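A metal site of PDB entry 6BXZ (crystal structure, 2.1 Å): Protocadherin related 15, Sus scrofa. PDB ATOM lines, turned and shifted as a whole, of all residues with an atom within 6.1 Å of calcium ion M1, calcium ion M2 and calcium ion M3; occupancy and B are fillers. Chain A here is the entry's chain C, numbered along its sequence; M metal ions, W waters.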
ATOM      1  N   GLU A  21      33.898 -11.505  22.260  1.00  0.00           N
ATOM      2  CA  GLU A  21      33.173 -12.637  21.674  1.00  0.00           C
ATOM      3  C   GLU A  21      33.222 -12.618  20.149  1.00  0.00           C
ATOM      4  O   GLU A  21      32.940 -13.649  19.536  1.00  0.00           O
ATOM      5  CB  GLU A  21      31.718 -12.685  22.139  1.00  0.00           C
ATOM      6  CG  GLU A  21      30.826 -11.594  21.547  1.00  0.00           C
ATOM      7  CD  GLU A  21      29.364 -11.720  21.972  1.00  0.00           C
ATOM      8  OE1 GLU A  21      28.701 -12.723  21.614  1.00  0.00           O
ATOM      9  OE2 GLU A  21      28.898 -10.778  22.639  1.00  0.00           O
ATOM     10  N   LEU A  22      33.537 -11.469  19.549  1.00  0.00           N
ATOM     11  CA  LEU A  22      33.746 -11.362  18.108  1.00  0.00           C
ATOM     12  C   LEU A  22      35.226 -11.490  17.709  1.00  0.00           C
ATOM     13  O   LEU A  22      35.589 -11.122  16.604  1.00  0.00           O
ATOM     14  CB  LEU A  22      33.217 -10.023  17.582  1.00  0.00           C
ATOM     15  CG  LEU A  22      31.766  -9.635  17.940  1.00  0.00           C
ATOM     16  CD1 LEU A  22      31.531  -8.150  17.639  1.00  0.00           C
ATOM     17  CD2 LEU A  22      30.761 -10.489  17.190  1.00  0.00           C
ATOM     18  N   LEU A  69      33.713 -17.573  19.109  1.00  0.00           N
ATOM     19  CA  LEU A  69      33.224 -17.431  20.486  1.00  0.00           C
ATOM     20  C   LEU A  69      31.807 -16.866  20.513  1.00  0.00           C
ATOM     21  O   LEU A  69      31.325 -16.314  19.532  1.00  0.00           O
ATOM     22  CB  LEU A  69      34.169 -16.544  21.293  1.00  0.00           C
ATOM     23  CG  LEU A  69      35.599 -17.075  21.477  1.00  0.00           C
ATOM     24  CD1 LEU A  69      36.484 -16.006  22.100  1.00  0.00           C
ATOM     25  CD2 LEU A  69      35.653 -18.353  22.305  1.00  0.00           C
ATOM     26  N   ASP A  70      31.142 -17.034  21.641  1.00  0.00           N
ATOM     27  CA  ASP A  70      29.802 -16.526  21.815  1.00  0.00           C
ATOM     28  C   ASP A  70      29.478 -16.352  23.298  1.00  0.00           C
ATOM     29  O   ASP A  70      29.224 -17.321  24.006  1.00  0.00           O
ATOM     30  CB  ASP A  70      28.789 -17.468  21.153  1.00  0.00           C
ATOM     31  CG  ASP A  70      27.355 -16.940  21.238  1.00  0.00           C
ATOM     32  OD1 ASP A  70      27.122 -15.724  21.396  1.00  0.00           O
ATOM     33  OD2 ASP A  70      26.432 -17.786  21.158  1.00  0.00           O
ATOM     34  N   TYR A  71      29.454 -15.095  23.722  1.00  0.00           N
ATOM     35  CA  TYR A  71      29.098 -14.735  25.103  1.00  0.00           C
ATOM     36  C   TYR A  71      27.735 -15.308  25.503  1.00  0.00           C
ATOM     37  O   TYR A  71      27.562 -15.723  26.644  1.00  0.00           O
ATOM     38  CB  TYR A  71      29.118 -13.218  25.258  1.00  0.00           C
ATOM     39  CG  TYR A  71      28.856 -12.761  26.662  1.00  0.00           C
ATOM     40  CD1 TYR A  71      27.547 -12.520  27.102  1.00  0.00           C
ATOM     41  CD2 TYR A  71      29.904 -12.564  27.556  1.00  0.00           C
ATOM     42  CE1 TYR A  71      27.298 -12.098  28.400  1.00  0.00           C
ATOM     43  CE2 TYR A  71      29.667 -12.140  28.861  1.00  0.00           C
ATOM     44  CZ  TYR A  71      28.368 -11.921  29.272  1.00  0.00           C
ATOM     45  OH  TYR A  71      28.127 -11.504  30.556  1.00  0.00           O
ATOM     46  N   GLU A  72      26.810 -15.347  24.545  1.00  0.00           N
ATOM     47  CA  GLU A  72      25.452 -15.833  24.801  1.00  0.00           C
ATOM     48  C   GLU A  72      25.339 -17.355  24.961  1.00  0.00           C
ATOM     49  O   GLU A  72      24.312 -17.841  25.417  1.00  0.00           O
ATOM     50  CB  GLU A  72      24.476 -15.321  23.714  1.00  0.00           C
ATOM     51  CG  GLU A  72      24.104 -13.846  23.830  1.00  0.00           C
ATOM     52  CD  GLU A  72      25.135 -12.857  23.309  1.00  0.00           C
ATOM     53  OE1 GLU A  72      25.365 -11.776  23.916  1.00  0.00           O
ATOM     54  OE2 GLU A  72      25.721 -13.115  22.241  1.00  0.00           O
ATOM     55  N   ASP A 110      31.136  -9.456  26.485  1.00  0.00           N
ATOM     56  CA  ASP A 110      29.916  -9.292  25.705  1.00  0.00           C
ATOM     57  C   ASP A 110      30.140  -8.161  24.698  1.00  0.00           C
ATOM     58  O   ASP A 110      30.623  -7.098  25.090  1.00  0.00           O
ATOM     59  CB  ASP A 110      28.740  -8.972  26.633  1.00  0.00           C
ATOM     60  CG  ASP A 110      27.413  -8.824  25.907  1.00  0.00           C
ATOM     61  OD1 ASP A 110      27.135  -9.555  24.920  1.00  0.00           O
ATOM     62  OD2 ASP A 110      26.622  -7.979  26.363  1.00  0.00           O
ATOM     63  N   GLU A 111      29.860  -8.435  23.426  1.00  0.00           N
ATOM     64  CA  GLU A 111      29.743  -7.402  22.407  1.00  0.00           C
ATOM     65  C   GLU A 111      28.284  -7.223  21.969  1.00  0.00           C
ATOM     66  O   GLU A 111      27.442  -8.106  22.176  1.00  0.00           O
ATOM     67  CB  GLU A 111      30.584  -7.700  21.174  1.00  0.00           C
ATOM     68  CG  GLU A 111      32.080  -7.928  21.449  1.00  0.00           C
ATOM     69  CD  GLU A 111      32.819  -6.747  22.054  1.00  0.00           C
ATOM     70  OE1 GLU A 111      32.275  -5.608  22.091  1.00  0.00           O
ATOM     71  OE2 GLU A 111      33.964  -6.973  22.506  1.00  0.00           O
ATOM     72  N   ASN A 112      28.044  -6.082  21.335  1.00  0.00           N
ATOM     73  CA  ASN A 112      26.697  -5.640  20.959  1.00  0.00           C
ATOM     74  C   ASN A 112      26.353  -6.257  19.604  1.00  0.00           C
ATOM     75  O   ASN A 112      26.509  -5.615  18.567  1.00  0.00           O
ATOM     76  CB  ASN A 112      26.610  -4.100  20.913  1.00  0.00           C
ATOM     77  CG  ASN A 112      25.181  -3.579  20.899  1.00  0.00           C
ATOM     78  OD1 ASN A 112      24.239  -4.343  21.045  1.00  0.00           O
ATOM     79  ND2 ASN A 112      25.032  -2.266  20.747  1.00  0.00           N
ATOM     80  N   ASP A 113      25.900  -7.509  19.625  1.00  0.00           N
ATOM     81  CA  ASP A 113      25.588  -8.248  18.399  1.00  0.00           C
ATOM     82  C   ASP A 113      24.132  -8.661  18.269  1.00  0.00           C
ATOM     83  O   ASP A 113      23.800  -9.462  17.406  1.00  0.00           O
ATOM     84  CB  ASP A 113      26.573  -9.435  18.167  1.00  0.00           C
ATOM     85  CG  ASP A 113      26.632 -10.457  19.323  1.00  0.00           C
ATOM     86  OD1 ASP A 113      26.080 -10.246  20.418  1.00  0.00           O
ATOM     87  OD2 ASP A 113      27.314 -11.513  19.123  1.00  0.00           O
ATOM     88  N   HIS A 114      23.245  -8.095  19.081  1.00  0.00           N
ATOM     89  CA  HIS A 114      21.817  -8.339  18.940  1.00  0.00           C
ATOM     90  C   HIS A 114      21.148  -6.975  18.900  1.00  0.00           C
ATOM     91  O   HIS A 114      21.335  -6.176  19.826  1.00  0.00           O
ATOM     92  CB  HIS A 114      21.293  -9.186  20.110  1.00  0.00           C
ATOM     93  CG  HIS A 114      21.852 -10.567  20.162  1.00  0.00           C
ATOM     94  ND1 HIS A 114      21.203 -11.663  19.622  1.00  0.00           N
ATOM     95  CD2 HIS A 114      23.000 -11.036  20.710  1.00  0.00           C
ATOM     96  CE1 HIS A 114      21.945 -12.735  19.816  1.00  0.00           C
ATOM     97  NE2 HIS A 114      23.024 -12.396  20.486  1.00  0.00           N
ATOM     98  N   PRO A 115      20.376  -6.683  17.830  1.00  0.00           N
ATOM     99  CA  PRO A 115      19.653  -5.407  17.844  1.00  0.00           C
ATOM    100  C   PRO A 115      18.411  -5.483  18.740  1.00  0.00           C
ATOM    101  O   PRO A 115      17.892  -6.568  18.958  1.00  0.00           O
ATOM    102  CB  PRO A 115      19.243  -5.236  16.364  1.00  0.00           C
ATOM    103  CG  PRO A 115      19.062  -6.629  15.881  1.00  0.00           C
ATOM    104  CD  PRO A 115      20.116  -7.449  16.588  1.00  0.00           C
ATOM    105  N   PRO A 116      17.910  -4.332  19.228  1.00  0.00           N
ATOM    106  CA  PRO A 116      16.621  -4.289  19.946  1.00  0.00           C
ATOM    107  C   PRO A 116      15.452  -4.911  19.150  1.00  0.00           C
ATOM    108  O   PRO A 116      15.359  -4.707  17.933  1.00  0.00           O
ATOM    109  CB  PRO A 116      16.399  -2.790  20.154  1.00  0.00           C
ATOM    110  CG  PRO A 116      17.773  -2.199  20.143  1.00  0.00           C
ATOM    111  CD  PRO A 116      18.499  -2.978  19.100  1.00  0.00           C
ATOM    112  N   ASP A 144      16.890  -7.152  24.100  1.00  0.00           N
ATOM    113  CA  ASP A 144      17.708  -8.055  23.290  1.00  0.00           C
ATOM    114  C   ASP A 144      18.593  -8.893  24.203  1.00  0.00           C
ATOM    115  O   ASP A 144      18.709  -8.627  25.389  1.00  0.00           O
ATOM    116  CB  ASP A 144      18.431  -7.348  22.121  1.00  0.00           C
ATOM    117  CG  ASP A 144      19.546  -6.388  22.552  1.00  0.00           C
ATOM    118  OD1 ASP A 144      20.655  -6.836  22.953  1.00  0.00           O
ATOM    119  OD2 ASP A 144      19.379  -5.154  22.381  1.00  0.00           O
ATOM    120  N   LYS A 145      19.208  -9.899  23.608  1.00  0.00           N
ATOM    121  CA  LYS A 145      19.943 -10.913  24.368  1.00  0.00           C
ATOM    122  C   LYS A 145      21.293 -10.470  24.919  1.00  0.00           C
ATOM    123  O   LYS A 145      21.885 -11.213  25.701  1.00  0.00           O
ATOM    124  CB  LYS A 145      20.133 -12.191  23.527  1.00  0.00           C
ATOM    125  CG  LYS A 145      18.877 -12.656  22.802  1.00  0.00           C
ATOM    126  CD  LYS A 145      18.837 -14.137  22.519  1.00  0.00           C
ATOM    127  CE  LYS A 145      17.580 -14.446  21.721  1.00  0.00           C
ATOM    128  NZ  LYS A 145      17.521 -15.890  21.325  1.00  0.00           N
ATOM    129  N   ASP A 146      21.785  -9.274  24.565  1.00  0.00           N
ATOM    130  CA  ASP A 146      23.047  -8.763  25.111  1.00  0.00           C
ATOM    131  C   ASP A 146      22.861  -8.382  26.563  1.00  0.00           C
ATOM    132  O   ASP A 146      21.745  -8.316  27.055  1.00  0.00           O
ATOM    133  CB  ASP A 146      23.541  -7.555  24.304  1.00  0.00           C
ATOM    134  CG  ASP A 146      23.853  -7.888  22.846  1.00  0.00           C
ATOM    135  OD1 ASP A 146      24.461  -8.932  22.613  1.00  0.00           O
ATOM    136  OD2 ASP A 146      23.506  -7.116  21.926  1.00  0.00           O
ATOM    137  N   THR A 147      23.962  -8.086  27.248  1.00  0.00           N
ATOM    138  CA  THR A 147      23.957  -7.766  28.665  1.00  0.00           C
ATOM    139  C   THR A 147      24.239  -6.291  28.902  1.00  0.00           C
ATOM    140  O   THR A 147      24.847  -5.609  28.050  1.00  0.00           O
ATOM    141  CB  THR A 147      25.049  -8.581  29.392  1.00  0.00           C
ATOM    142  OG1 THR A 147      24.873  -9.977  29.113  1.00  0.00           O
ATOM    143  CG2 THR A 147      25.036  -8.348  30.910  1.00  0.00           C
ATOM    144  N   TYR A 150      24.558  -2.932  26.534  1.00  0.00           N
ATOM    145  CA  TYR A 150      24.275  -3.406  25.174  1.00  0.00           C
ATOM    146  C   TYR A 150      22.852  -3.920  24.889  1.00  0.00           C
ATOM    147  O   TYR A 150      22.523  -4.252  23.727  1.00  0.00           O
ATOM    148  CB  TYR A 150      25.346  -4.430  24.730  1.00  0.00           C
ATOM    149  CG  TYR A 150      26.744  -3.849  24.569  1.00  0.00           C
ATOM    150  CD1 TYR A 150      26.953  -2.503  24.217  1.00  0.00           C
ATOM    151  CD2 TYR A 150      27.876  -4.658  24.742  1.00  0.00           C
ATOM    152  CE1 TYR A 150      28.224  -1.993  24.056  1.00  0.00           C
ATOM    153  CE2 TYR A 150      29.154  -4.136  24.580  1.00  0.00           C
ATOM    154  CZ  TYR A 150      29.321  -2.808  24.237  1.00  0.00           C
ATOM    155  OH  TYR A 150      30.542  -2.265  24.070  1.00  0.00           O
ATOM    156  N   SER A 151      22.012  -3.987  25.937  1.00  0.00           N
ATOM    157  CA  SER A 151      20.575  -4.134  25.752  1.00  0.00           C
ATOM    158  C   SER A 151      19.761  -3.090  26.560  1.00  0.00           C
ATOM    159  O   SER A 151      18.601  -3.319  26.839  1.00  0.00           O
ATOM    160  CB  SER A 151      20.146  -5.542  26.143  1.00  0.00           C
ATOM    161  OG  SER A 151      20.408  -5.755  27.516  1.00  0.00           O
ATOM    162  N   MET A 153      17.982   0.416  26.662  1.00  0.00           N
ATOM    163  CA  MET A 153      17.345   1.113  25.550  1.00  0.00           C
ATOM    164  C   MET A 153      17.165   2.607  25.771  1.00  0.00           C
ATOM    165  O   MET A 153      16.830   3.025  26.867  1.00  0.00           O
ATOM    166  CB  MET A 153      15.961   0.494  25.315  1.00  0.00           C
ATOM    167  CG  MET A 153      15.984  -0.995  25.023  1.00  0.00           C
ATOM    168  SD  MET A 153      17.007  -1.407  23.600  1.00  0.00           S
ATOM    169  CE  MET A 153      17.081  -3.199  23.715  1.00  0.00           C
ATOM    170  N   ASP A 200      19.910   0.567  21.546  1.00  0.00           N
ATOM    171  CA  ASP A 200      20.619   0.075  22.736  1.00  0.00           C
ATOM    172  C   ASP A 200      21.900   0.888  22.971  1.00  0.00           C
ATOM    173  O   ASP A 200      22.238   1.805  22.211  1.00  0.00           O
ATOM    174  CB  ASP A 200      20.873  -1.435  22.654  1.00  0.00           C
ATOM    175  CG  ASP A 200      21.697  -1.835  21.452  1.00  0.00           C
ATOM    176  OD1 ASP A 200      22.551  -1.047  20.991  1.00  0.00           O
ATOM    177  OD2 ASP A 200      21.459  -2.939  20.930  1.00  0.00           O
ATOM    178  N   LEU A 206      22.745  -0.296  18.392  1.00  0.00           N
ATOM    179  CA  LEU A 206      21.890  -0.834  17.341  1.00  0.00           C
ATOM    180  C   LEU A 206      20.428  -0.460  17.600  1.00  0.00           C
ATOM    181  O   LEU A 206      20.048  -0.176  18.729  1.00  0.00           O
ATOM    182  CB  LEU A 206      22.027  -2.356  17.271  1.00  0.00           C
ATOM    183  CG  LEU A 206      23.432  -2.954  17.032  1.00  0.00           C
ATOM    184  CD1 LEU A 206      23.407  -4.474  17.132  1.00  0.00           C
ATOM    185  CD2 LEU A 206      23.989  -2.519  15.691  1.00  0.00           C
HETATM  186 CA    CA M   1      26.980 -13.627  20.308  1.00  0.00          CA
HETATM  187 CA    CA M   2      26.505 -10.112  22.819  1.00  0.00          CA
HETATM  188 CA    CA M   3      22.056  -5.088  21.673  1.00  0.00          CA
HETATM  189  O   HOH W   1      28.749 -14.374  18.748  1.00  0.00           O
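A ring nitrogen (NE2) of His 114 lies close to the side-chain carboxylate of Glu 72, at 3.3 Å. The backbone carbonyl oxygen of Asp 146 is in hydrogen-bond range of the side-chain hydroxyl of Ser 151. The side-chain carboxylate of Asp 200 sits at hydrogen-bond distance from the backbone NH of Leu 206. The backbone NH (N) of Tyr 71 sits close to the side-chain carboxylate (OE1) of Glu 21 (3.3 Å). The side-chain carboxylate (OD2) of Asp 110 sits at hydrogen-bond distance from the backbone NH (N) of Thr 147, at 2.8 Å.
Within 4 Å of calcium ion M1: Glu 21, Asp 70, Glu 72 and Asp 113. The nearest printed residue that does not touch calcium ion M1 is His 114 (4.1 Å).
Within 4 Å of calcium ion M2: Glu 21, Glu 72, Asp 110, Glu 111, Asp 113 and Asp 146.
Six residues have an atom within 4 Å of calcium ion M3: Asn 112, His 114, Asp 144, Asp 146, Tyr 150 and Asp 200. Along chain A the residues within 4 Å of calcium ion M3 span positions 112 to 200. The nearest printed residue that does not touch calcium ion M3 is Ser 151 (4.4 Å).
Calcium ion M1 is bound by OE1 of Glu 21, at 2.3 Å. OE2 of Glu 72 binds calcium ion M1, 2.4 Å away. OD1 of Asp 70 is bound to calcium ion M1, 2.4 Å away. Calcium ion M1 is bound by OD2 of Asp 113 (2.4 Å). Water W1 binds calcium ion M1, at 2.5 Å.
Calcium ion M2 is bound by OD1 of Asp 110 (2.3 Å), OE1 of Glu 72 (2.3 Å), O of Glu 111 (2.3 Å), OD1 of Asp 146 (2.4 Å), OD1 of Asp 113 (2.4 Å) and OE2 of Glu 21 (2.5 Å). Calcium ion M2 has six donor atoms within binding distance.
Calcium ion M3 is bound by O of His 114 (2.3 Å), O of Tyr 150 (2.3 Å), OD2 of Asp 200 (2.4 Å), OD1 of Asn 112 (2.4 Å), OD2 of Asp 146 (2.5 Å), OD1 of Asp 144 (2.6 Å) and OD2 of Asp 144 (2.8 Å).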
